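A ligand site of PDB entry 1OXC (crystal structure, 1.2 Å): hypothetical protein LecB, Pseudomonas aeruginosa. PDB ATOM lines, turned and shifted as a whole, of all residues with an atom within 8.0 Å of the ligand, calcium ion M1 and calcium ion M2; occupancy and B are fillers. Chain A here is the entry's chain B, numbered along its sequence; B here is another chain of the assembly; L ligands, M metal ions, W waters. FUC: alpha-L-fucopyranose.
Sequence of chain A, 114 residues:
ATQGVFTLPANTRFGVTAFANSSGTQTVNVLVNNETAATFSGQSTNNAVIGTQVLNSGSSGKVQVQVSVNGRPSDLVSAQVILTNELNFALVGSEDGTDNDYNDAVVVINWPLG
The nearest printed residue that does not touch calcium ion M2 is Ser 22 (4.4 Å).
Calcium ion M1 is bound by OD1 of Asp 99 (2.3 Å), OD1 of Asp 101 (2.4 Å), OE2 of Glu 95 (2.4 Å), OD2 of Asp 104 (2.4 Å), OE1 of Glu 95 (2.5 Å), O2 of the ligand (2.5 Å), O3 of the ligand (2.5 Å) and OD1 of Asp 104 (2.6 Å). Calcium ion M1 has eight donor atoms within binding distance.
Water W2 bridges an oxygen (O1) of the ligand and the side-chain carboxylate of Asp 96. Water W1 bridges the side-chain carboxylate of Asp 96 and an oxygen (O1) of the ligand.
The side-chain carboxylate (OD1) of Asp 96 is in hydrogen-bond range of an oxygen (O1) of the ligand, at 3.2 Å. The side-chain hydroxyl (OG) of Ser 22 lies within hydrogen-bond range of an oxygen (O1) of the ligand (2.7 Å). N of Ser 23 lies within hydrogen-bond range of O5 of the ligand (2.9 Å). OG of Ser 23 sits at hydrogen-bond distance from O5 of the ligand, at 3.1 Å.
OD1 of Asn 103 is bound to calcium ion M2, 2.3 Å away. O of Asn 21 binds calcium ion M2 (2.4 Å). OD2 of Asp 101 is bound to calcium ion M2. The side-chain carboxylate (OD1) of Asp 104 binds calcium ion M2, 2.4 Å away. Calcium ion M2 is bound by O of Gly 114 of chain B, at 2.4 Å. O3 of the ligand is bound to calcium ion M2 (2.5 Å). O4 of the ligand is bound to calcium ion M2 (2.5 Å). Calcium ion M2 has seven donor atoms within binding distance. Slightly farther from calcium ion M2 lies OD1 of Asp 101 (3.1 Å).
Of the 28 residues printed, 4 come within 4 Å of calcium ion M1.
The backbone NH (N) of Asn 103 lies within hydrogen-bond range of the backbone carbonyl oxygen (O) of Ser 94, at 3.4 Å. The side-chain amide nitrogen of Asn 103 sits close to the backbone carbonyl oxygen of Leu 113 of chain B, at 3.5 Å. N of Gly 97 lies close to OE2 of Glu 95. N of Tyr 102 lies close to OE1 of Glu 95. OD2 of Asp 104 sits close to N of Asp 96, at 2.8 Å. N of Asp 104 sits at hydrogen-bond distance from O of Ser 94 (3.2 Å). The side-chain carboxylate (OD2) of Asp 96 lies within hydrogen-bond range of the side-chain hydroxyl (OG) of Ser 22. NE2 of Gln 43 lies within hydrogen-bond range of O of Ser 22, 2.9 Å away.
Within 4 Å of the ligand: Asn 21, Ser 22, Ser 23, Glu 95, Asp 96, Asp 99, Asp 101, Asp 104 and Gly 114 of chain B. The nearest printed residue that does not touch the ligand is Gly 24 (4.03 Å).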
ATOM      1  N   ALA A  20     -20.568   1.189  16.106  1.00  0.00           N
ATOM      2  CA  ALA A  20     -19.882   1.773  17.264  1.00  0.00           C
ATOM      3  C   ALA A  20     -20.048   3.289  17.326  1.00  0.00           C
ATOM      4  O   ALA A  20     -19.974   3.984  16.305  1.00  0.00           O
ATOM      5  CB  ALA A  20     -18.402   1.403  17.221  1.00  0.00           C
ATOM      6  N   ASN A  21     -20.268   3.800  18.533  1.00  0.00           N
ATOM      7  CA  ASN A  21     -20.434   5.233  18.794  1.00  0.00           C
ATOM      8  C   ASN A  21     -19.883   5.513  20.185  1.00  0.00           C
ATOM      9  O   ASN A  21     -20.638   5.780  21.125  1.00  0.00           O
ATOM     10  CB  ASN A  21     -21.907   5.623  18.752  1.00  0.00           C
ATOM     11  CG  ASN A  21     -22.477   5.579  17.360  1.00  0.00           C
ATOM     12  OD1 ASN A  21     -22.233   6.467  16.536  1.00  0.00           O
ATOM     13  ND2 ASN A  21     -23.237   4.528  17.065  1.00  0.00           N
ATOM     14  N   SER A  22     -18.567   5.464  20.317  1.00  0.00           N
ATOM     15  CA  SER A  22     -17.929   5.685  21.609  1.00  0.00           C
ATOM     16  C   SER A  22     -16.431   5.890  21.456  1.00  0.00           C
ATOM     17  O   SER A  22     -15.840   5.478  20.459  1.00  0.00           O
ATOM     18  CB  SER A  22     -18.170   4.465  22.512  1.00  0.00           C
ATOM     19  OG  SER A  22     -17.447   4.570  23.725  1.00  0.00           O
ATOM     20  N   SER A  23     -15.828   6.544  22.434  1.00  0.00           N
ATOM     21  CA  SER A  23     -14.393   6.781  22.423  1.00  0.00           C
ATOM     22  C   SER A  23     -13.683   5.478  22.780  1.00  0.00           C
ATOM     23  O   SER A  23     -12.504   5.317  22.494  1.00  0.00           O
ATOM     24  CB  SER A  23     -14.034   7.863  23.457  1.00  0.00           C
ATOM     25  OG  SER A  23     -14.459   7.475  24.752  1.00  0.00           O
ATOM     26  N   GLY A  24     -14.412   4.562  23.394  1.00  0.00           N
ATOM     27  CA  GLY A  24     -13.830   3.288  23.787  1.00  0.00           C
ATOM     28  C   GLY A  24     -13.997   2.200  22.742  1.00  0.00           C
ATOM     29  O   GLY A  24     -14.993   2.165  22.013  1.00  0.00           O
ATOM     30  N   THR A  25     -13.016   1.300  22.673  1.00  0.00           N
ATOM     31  CA  THR A  25     -13.068   0.195  21.720  1.00  0.00           C
ATOM     32  C   THR A  25     -14.132  -0.786  22.164  1.00  0.00           C
ATOM     33  O   THR A  25     -14.117  -1.290  23.288  1.00  0.00           O
ATOM     34  CB  THR A  25     -11.704  -0.517  21.640  1.00  0.00           C
ATOM     35  OG1 THR A  25     -10.704   0.406  21.195  1.00  0.00           O
ATOM     36  CG2 THR A  25     -11.774  -1.696  20.686  1.00  0.00           C
ATOM     37  N   GLN A  26     -15.070  -1.066  21.268  1.00  0.00           N
ATOM     38  CA  GLN A  26     -16.169  -1.978  21.552  1.00  0.00           C
ATOM     39  C   GLN A  26     -15.847  -3.388  21.122  1.00  0.00           C
ATOM     40  O   GLN A  26     -15.155  -3.602  20.131  1.00  0.00           O
ATOM     41  CB  GLN A  26     -17.417  -1.539  20.783  1.00  0.00           C
ATOM     42  CG  GLN A  26     -17.858  -0.113  21.039  1.00  0.00           C
ATOM     43  CD  GLN A  26     -18.261   0.130  22.474  1.00  0.00           C
ATOM     44  OE1 GLN A  26     -19.137  -0.553  22.997  1.00  0.00           O
ATOM     45  NE2 GLN A  26     -17.626   1.102  23.108  1.00  0.00           N
ATOM     46  N   GLN A  43     -13.492   0.882  16.948  1.00  0.00           N
ATOM     47  CA  GLN A  43     -13.593   2.126  17.696  1.00  0.00           C
ATOM     48  C   GLN A  43     -13.969   3.243  16.741  1.00  0.00           C
ATOM     49  O   GLN A  43     -13.201   3.612  15.847  1.00  0.00           O
ATOM     50  CB  GLN A  43     -12.268   2.444  18.393  1.00  0.00           C
ATOM     51  CG  GLN A  43     -12.323   3.674  19.312  1.00  0.00           C
ATOM     52  CD  GLN A  43     -12.410   4.984  18.554  1.00  0.00           C
ATOM     53  OE1 GLN A  43     -11.561   5.278  17.706  1.00  0.00           O
ATOM     54  NE2 GLN A  43     -13.427   5.788  18.861  1.00  0.00           N
ATOM     55  N   SER A  44     -15.163   3.774  16.942  1.00  0.00           N
ATOM     56  CA  SER A  44     -15.697   4.847  16.116  1.00  0.00           C
ATOM     57  C   SER A  44     -16.715   5.654  16.915  1.00  0.00           C
ATOM     58  O   SER A  44     -17.413   5.116  17.769  1.00  0.00           O
ATOM     59  CB  SER A  44     -16.403   4.253  14.889  1.00  0.00           C
ATOM     60  OG  SER A  44     -17.124   5.227  14.152  1.00  0.00           O
ATOM     61  N   THR A  45     -16.778   6.956  16.635  1.00  0.00           N
ATOM     62  CA  THR A  45     -17.755   7.827  17.265  1.00  0.00           C
ATOM     63  C   THR A  45     -18.672   8.301  16.150  1.00  0.00           C
ATOM     64  O   THR A  45     -19.440   9.256  16.311  1.00  0.00           O
ATOM     65  CB  THR A  45     -17.111   9.045  17.962  1.00  0.00           C
ATOM     66  OG1 THR A  45     -16.181   9.680  17.075  1.00  0.00           O
ATOM     67  CG2 THR A  45     -16.400   8.613  19.233  1.00  0.00           C
ATOM     68  N   ASN A  46     -18.600   7.606  15.011  1.00  0.00           N
ATOM     69  CA  ASN A  46     -19.402   7.954  13.850  1.00  0.00           C
ATOM     70  C   ASN A  46     -20.187   6.803  13.222  1.00  0.00           C
ATOM     71  O   ASN A  46     -20.345   6.730  12.005  1.00  0.00           O
ATOM     72  CB  ASN A  46     -18.509   8.651  12.820  1.00  0.00           C
ATOM     73  CG  ASN A  46     -18.073  10.027  13.280  1.00  0.00           C
ATOM     74  OD1 ASN A  46     -18.863  10.977  13.271  1.00  0.00           O
ATOM     75  ND2 ASN A  46     -16.822  10.142  13.708  1.00  0.00           N
ATOM     76  N   VAL A  69     -16.196  -3.517  26.924  1.00  0.00           N
ATOM     77  CA  VAL A  69     -15.199  -2.501  26.598  1.00  0.00           C
ATOM     78  C   VAL A  69     -14.044  -2.734  27.557  1.00  0.00           C
ATOM     79  O   VAL A  69     -14.200  -2.608  28.773  1.00  0.00           O
ATOM     80  CB  VAL A  69     -15.772  -1.083  26.793  1.00  0.00           C
ATOM     81  CG1 VAL A  69     -14.696  -0.051  26.498  1.00  0.00           C
ATOM     82  CG2 VAL A  69     -16.968  -0.876  25.869  1.00  0.00           C
ATOM     83  N   SER A  94     -26.236  -0.507  23.953  1.00  0.00           N
ATOM     84  CA  SER A  94     -25.372  -0.727  25.106  1.00  0.00           C
ATOM     85  C   SER A  94     -24.736   0.566  25.574  1.00  0.00           C
ATOM     86  O   SER A  94     -24.489   1.484  24.789  1.00  0.00           O
ATOM     87  CB  SER A  94     -24.283  -1.755  24.787  1.00  0.00           C
ATOM     88  OG  SER A  94     -23.418  -1.284  23.774  1.00  0.00           O
ATOM     89  N   GLU A  95     -24.479   0.639  26.875  1.00  0.00           N
ATOM     90  CA  GLU A  95     -23.875   1.827  27.473  1.00  0.00           C
ATOM     91  C   GLU A  95     -22.601   1.437  28.221  1.00  0.00           C
ATOM     92  O   GLU A  95     -22.641   0.604  29.141  1.00  0.00           O
ATOM     93  CB  GLU A  95     -24.886   2.485  28.414  1.00  0.00           C
ATOM     94  CG  GLU A  95     -24.361   3.712  29.147  1.00  0.00           C
ATOM     95  CD  GLU A  95     -23.801   4.755  28.207  1.00  0.00           C
ATOM     96  OE1 GLU A  95     -24.524   5.181  27.279  1.00  0.00           O
ATOM     97  OE2 GLU A  95     -22.626   5.141  28.388  1.00  0.00           O
ATOM     98  N   ASP A  96     -21.481   2.028  27.817  1.00  0.00           N
ATOM     99  CA  ASP A  96     -20.195   1.732  28.441  1.00  0.00           C
ATOM    100  C   ASP A  96     -19.759   2.808  29.428  1.00  0.00           C
ATOM    101  O   ASP A  96     -18.653   2.746  29.982  1.00  0.00           O
ATOM    102  CB  ASP A  96     -19.095   1.579  27.379  1.00  0.00           C
ATOM    103  CG  ASP A  96     -18.856   2.857  26.582  1.00  0.00           C
ATOM    104  OD1 ASP A  96     -19.113   3.962  27.093  1.00  0.00           O
ATOM    105  OD2 ASP A  96     -18.373   2.748  25.433  1.00  0.00           O
ATOM    106  N   GLY A  97     -20.624   3.792  29.654  1.00  0.00           N
ATOM    107  CA  GLY A  97     -20.297   4.879  30.560  1.00  0.00           C
ATOM    108  C   GLY A  97     -21.491   5.358  31.356  1.00  0.00           C
ATOM    109  O   GLY A  97     -22.294   4.553  31.822  1.00  0.00           O
ATOM    110  N   THR A  98     -21.622   6.669  31.498  1.00  0.00           N
ATOM    111  CA  THR A  98     -22.717   7.246  32.274  1.00  0.00           C
ATOM    112  C   THR A  98     -23.479   8.375  31.587  1.00  0.00           C
ATOM    113  O   THR A  98     -24.319   9.020  32.215  1.00  0.00           O
ATOM    114  CB  THR A  98     -22.188   7.782  33.621  1.00  0.00           C
ATOM    115  OG1 THR A  98     -21.205   8.794  33.367  1.00  0.00           O
ATOM    116  CG2 THR A  98     -21.540   6.662  34.426  1.00  0.00           C
ATOM    117  N   ASP A  99     -23.196   8.627  30.304  1.00  0.00           N
ATOM    118  CA  ASP A  99     -23.889   9.707  29.601  1.00  0.00           C
ATOM    119  C   ASP A  99     -25.232   9.233  29.064  1.00  0.00           C
ATOM    120  O   ASP A  99     -25.987   9.992  28.467  1.00  0.00           O
ATOM    121  CB  ASP A  99     -23.001  10.242  28.466  1.00  0.00           C
ATOM    122  CG  ASP A  99     -22.921   9.300  27.290  1.00  0.00           C
ATOM    123  OD1 ASP A  99     -22.943   8.066  27.503  1.00  0.00           O
ATOM    124  OD2 ASP A  99     -22.802   9.803  26.154  1.00  0.00           O
ATOM    125  N   ASN A 100     -25.508   7.952  29.308  1.00  0.00           N
ATOM    126  CA  ASN A 100     -26.747   7.308  28.919  1.00  0.00           C
ATOM    127  C   ASN A 100     -27.285   7.555  27.511  1.00  0.00           C
ATOM    128  O   ASN A 100     -28.442   7.953  27.349  1.00  0.00           O
ATOM    129  CB  ASN A 100     -27.829   7.631  29.952  1.00  0.00           C
ATOM    130  CG  ASN A 100     -27.500   7.066  31.325  1.00  0.00           C
ATOM    131  OD1 ASN A 100     -28.213   7.304  32.297  1.00  0.00           O
ATOM    132  ND2 ASN A 100     -26.417   6.297  31.407  1.00  0.00           N
ATOM    133  N   ASP A 101     -26.462   7.318  26.506  1.00  0.00           N
ATOM    134  CA  ASP A 101     -26.956   7.446  25.144  1.00  0.00           C
ATOM    135  C   ASP A 101     -27.209   6.036  24.603  1.00  0.00           C
ATOM    136  O   ASP A 101     -27.918   5.866  23.611  1.00  0.00           O
ATOM    137  CB  ASP A 101     -26.032   8.294  24.242  1.00  0.00           C
ATOM    138  CG  ASP A 101     -24.624   7.742  24.083  1.00  0.00           C
ATOM    139  OD1 ASP A 101     -24.243   6.773  24.765  1.00  0.00           O
ATOM    140  OD2 ASP A 101     -23.891   8.309  23.246  1.00  0.00           O
ATOM    141  N   TYR A 102     -26.668   5.029  25.281  1.00  0.00           N
ATOM    142  CA  TYR A 102     -26.888   3.628  24.925  1.00  0.00           C
ATOM    143  C   TYR A 102     -26.635   3.232  23.474  1.00  0.00           C
ATOM    144  O   TYR A 102     -27.197   2.261  22.978  1.00  0.00           O
ATOM    145  CB  TYR A 102     -28.303   3.221  25.348  1.00  0.00           C
ATOM    146  CG  TYR A 102     -28.385   2.889  26.811  1.00  0.00           C
ATOM    147  CD1 TYR A 102     -28.152   1.584  27.253  1.00  0.00           C
ATOM    148  CD2 TYR A 102     -28.587   3.886  27.765  1.00  0.00           C
ATOM    149  CE1 TYR A 102     -28.094   1.291  28.614  1.00  0.00           C
ATOM    150  CE2 TYR A 102     -28.530   3.593  29.126  1.00  0.00           C
ATOM    151  CZ  TYR A 102     -28.278   2.303  29.539  1.00  0.00           C
ATOM    152  OH  TYR A 102     -28.194   2.008  30.885  1.00  0.00           O
ATOM    153  N   ASN A 103     -25.750   3.962  22.808  1.00  0.00           N
ATOM    154  CA  ASN A 103     -25.437   3.687  21.403  1.00  0.00           C
ATOM    155  C   ASN A 103     -23.969   3.318  21.245  1.00  0.00           C
ATOM    156  O   ASN A 103     -23.483   3.205  20.121  1.00  0.00           O
ATOM    157  CB  ASN A 103     -25.685   4.944  20.581  1.00  0.00           C
ATOM    158  CG  ASN A 103     -24.667   6.029  20.871  1.00  0.00           C
ATOM    159  OD1 ASN A 103     -23.818   5.870  21.744  1.00  0.00           O
ATOM    160  ND2 ASN A 103     -24.738   7.139  20.141  1.00  0.00           N
ATOM    161  N   ASP A 104     -23.267   3.115  22.362  1.00  0.00           N
ATOM    162  CA  ASP A 104     -21.841   2.848  22.296  1.00  0.00           C
ATOM    163  C   ASP A 104     -21.500   1.680  21.395  1.00  0.00           C
ATOM    164  O   ASP A 104     -20.530   1.720  20.637  1.00  0.00           O
ATOM    165  CB  ASP A 104     -21.301   2.719  23.714  1.00  0.00           C
ATOM    166  CG  ASP A 104     -21.639   3.945  24.558  1.00  0.00           C
ATOM    167  OD1 ASP A 104     -21.575   5.073  24.007  1.00  0.00           O
ATOM    168  OD2 ASP A 104     -21.970   3.809  25.750  1.00  0.00           O
ATOM    169  N   ALA A 105     -22.346   0.661  21.452  1.00  0.00           N
ATOM    170  CA  ALA A 105     -22.269  -0.493  20.580  1.00  0.00           C
ATOM    171  C   ALA A 105     -23.740  -0.801  20.330  1.00  0.00           C
ATOM    172  O   ALA A 105     -24.504  -1.012  21.269  1.00  0.00           O
ATOM    173  CB  ALA A 105     -21.585  -1.673  21.259  1.00  0.00           C
ATOM    174  N   GLU B  86     -34.629   6.637  25.057  1.00  0.00           N
ATOM    175  CA  GLU B  86     -33.558   7.451  24.490  1.00  0.00           C
ATOM    176  C   GLU B  86     -32.884   6.914  23.221  1.00  0.00           C
ATOM    177  O   GLU B  86     -32.450   7.689  22.374  1.00  0.00           O
ATOM    178  CB  GLU B  86     -32.520   7.720  25.584  1.00  0.00           C
ATOM    179  CG  GLU B  86     -31.473   8.767  25.241  1.00  0.00           C
ATOM    180  CD  GLU B  86     -30.335   8.214  24.418  1.00  0.00           C
ATOM    181  OE1 GLU B  86     -29.527   9.023  23.923  1.00  0.00           O
ATOM    182  OE2 GLU B  86     -30.240   6.975  24.288  1.00  0.00           O
ATOM    183  N   PRO B 112     -29.401   8.372  18.834  1.00  0.00           N
ATOM    184  CA  PRO B 112     -28.339   9.310  18.467  1.00  0.00           C
ATOM    185  C   PRO B 112     -27.047   8.600  18.101  1.00  0.00           C
ATOM    186  O   PRO B 112     -26.882   7.393  18.346  1.00  0.00           O
ATOM    187  CB  PRO B 112     -28.164  10.107  19.748  1.00  0.00           C
ATOM    188  CG  PRO B 112     -28.313   9.014  20.786  1.00  0.00           C
ATOM    189  CD  PRO B 112     -29.614   8.390  20.294  1.00  0.00           C
ATOM    190  N   LEU B 113     -26.124   9.353  17.513  1.00  0.00           N
ATOM    191  CA  LEU B 113     -24.811   8.835  17.158  1.00  0.00           C
ATOM    192  C   LEU B 113     -23.817   9.516  18.099  1.00  0.00           C
ATOM    193  O   LEU B 113     -24.209  10.357  18.916  1.00  0.00           O
ATOM    194  CB  LEU B 113     -24.453   9.189  15.720  1.00  0.00           C
ATOM    195  CG  LEU B 113     -25.411   8.729  14.623  1.00  0.00           C
ATOM    196  CD1 LEU B 113     -24.794   9.046  13.264  1.00  0.00           C
ATOM    197  CD2 LEU B 113     -25.668   7.244  14.749  1.00  0.00           C
ATOM    198  N   GLY B 114     -22.552   9.137  17.976  1.00  0.00           N
ATOM    199  CA  GLY B 114     -21.496   9.736  18.779  1.00  0.00           C
ATOM    200  C   GLY B 114     -21.243   9.186  20.160  1.00  0.00           C
ATOM    201  O   GLY B 114     -22.087   8.449  20.703  1.00  0.00           O
ATOM    202  OXT GLY B 114     -20.176   9.517  20.723  1.00  0.00           O
HETATM  203  C1  FUC L   1     -17.857   7.258  25.548  1.00  0.00           C
HETATM  204  C2  FUC L   1     -19.548   6.967  25.361  1.00  0.00           C
HETATM  205  C3  FUC L   1     -20.221   8.318  25.174  1.00  0.00           C
HETATM  206  C4  FUC L   1     -19.590   9.032  24.023  1.00  0.00           C
HETATM  207  C5  FUC L   1     -18.106   9.205  24.308  1.00  0.00           C
HETATM  208  C6  FUC L   1     -17.455   9.914  23.170  1.00  0.00           C
HETATM  209  O1  FUC L   1     -17.181   6.210  25.821  1.00  0.00           O
HETATM  210  O2  FUC L   1     -20.040   6.415  26.567  1.00  0.00           O
HETATM  211  O3  FUC L   1     -21.599   8.104  24.895  1.00  0.00           O
HETATM  212  O4  FUC L   1     -19.769   8.252  22.849  1.00  0.00           O
HETATM  213  O5  FUC L   1     -17.463   7.915  24.421  1.00  0.00           O
HETATM  214 CA    CA M   1     -22.515   6.146  26.234  1.00  0.00          CA
HETATM  215 CA    CA M   2     -21.981   7.015  22.647  1.00  0.00          CA
HETATM  216  O   HOH W   1     -15.580   3.600  26.692  1.00  0.00           O
HETATM  217  O   HOH W   2     -16.885   5.479  28.241  1.00  0.00           O
HETATM  218  O   HOH W   3     -20.114   8.070  29.159  1.00  0.00           O
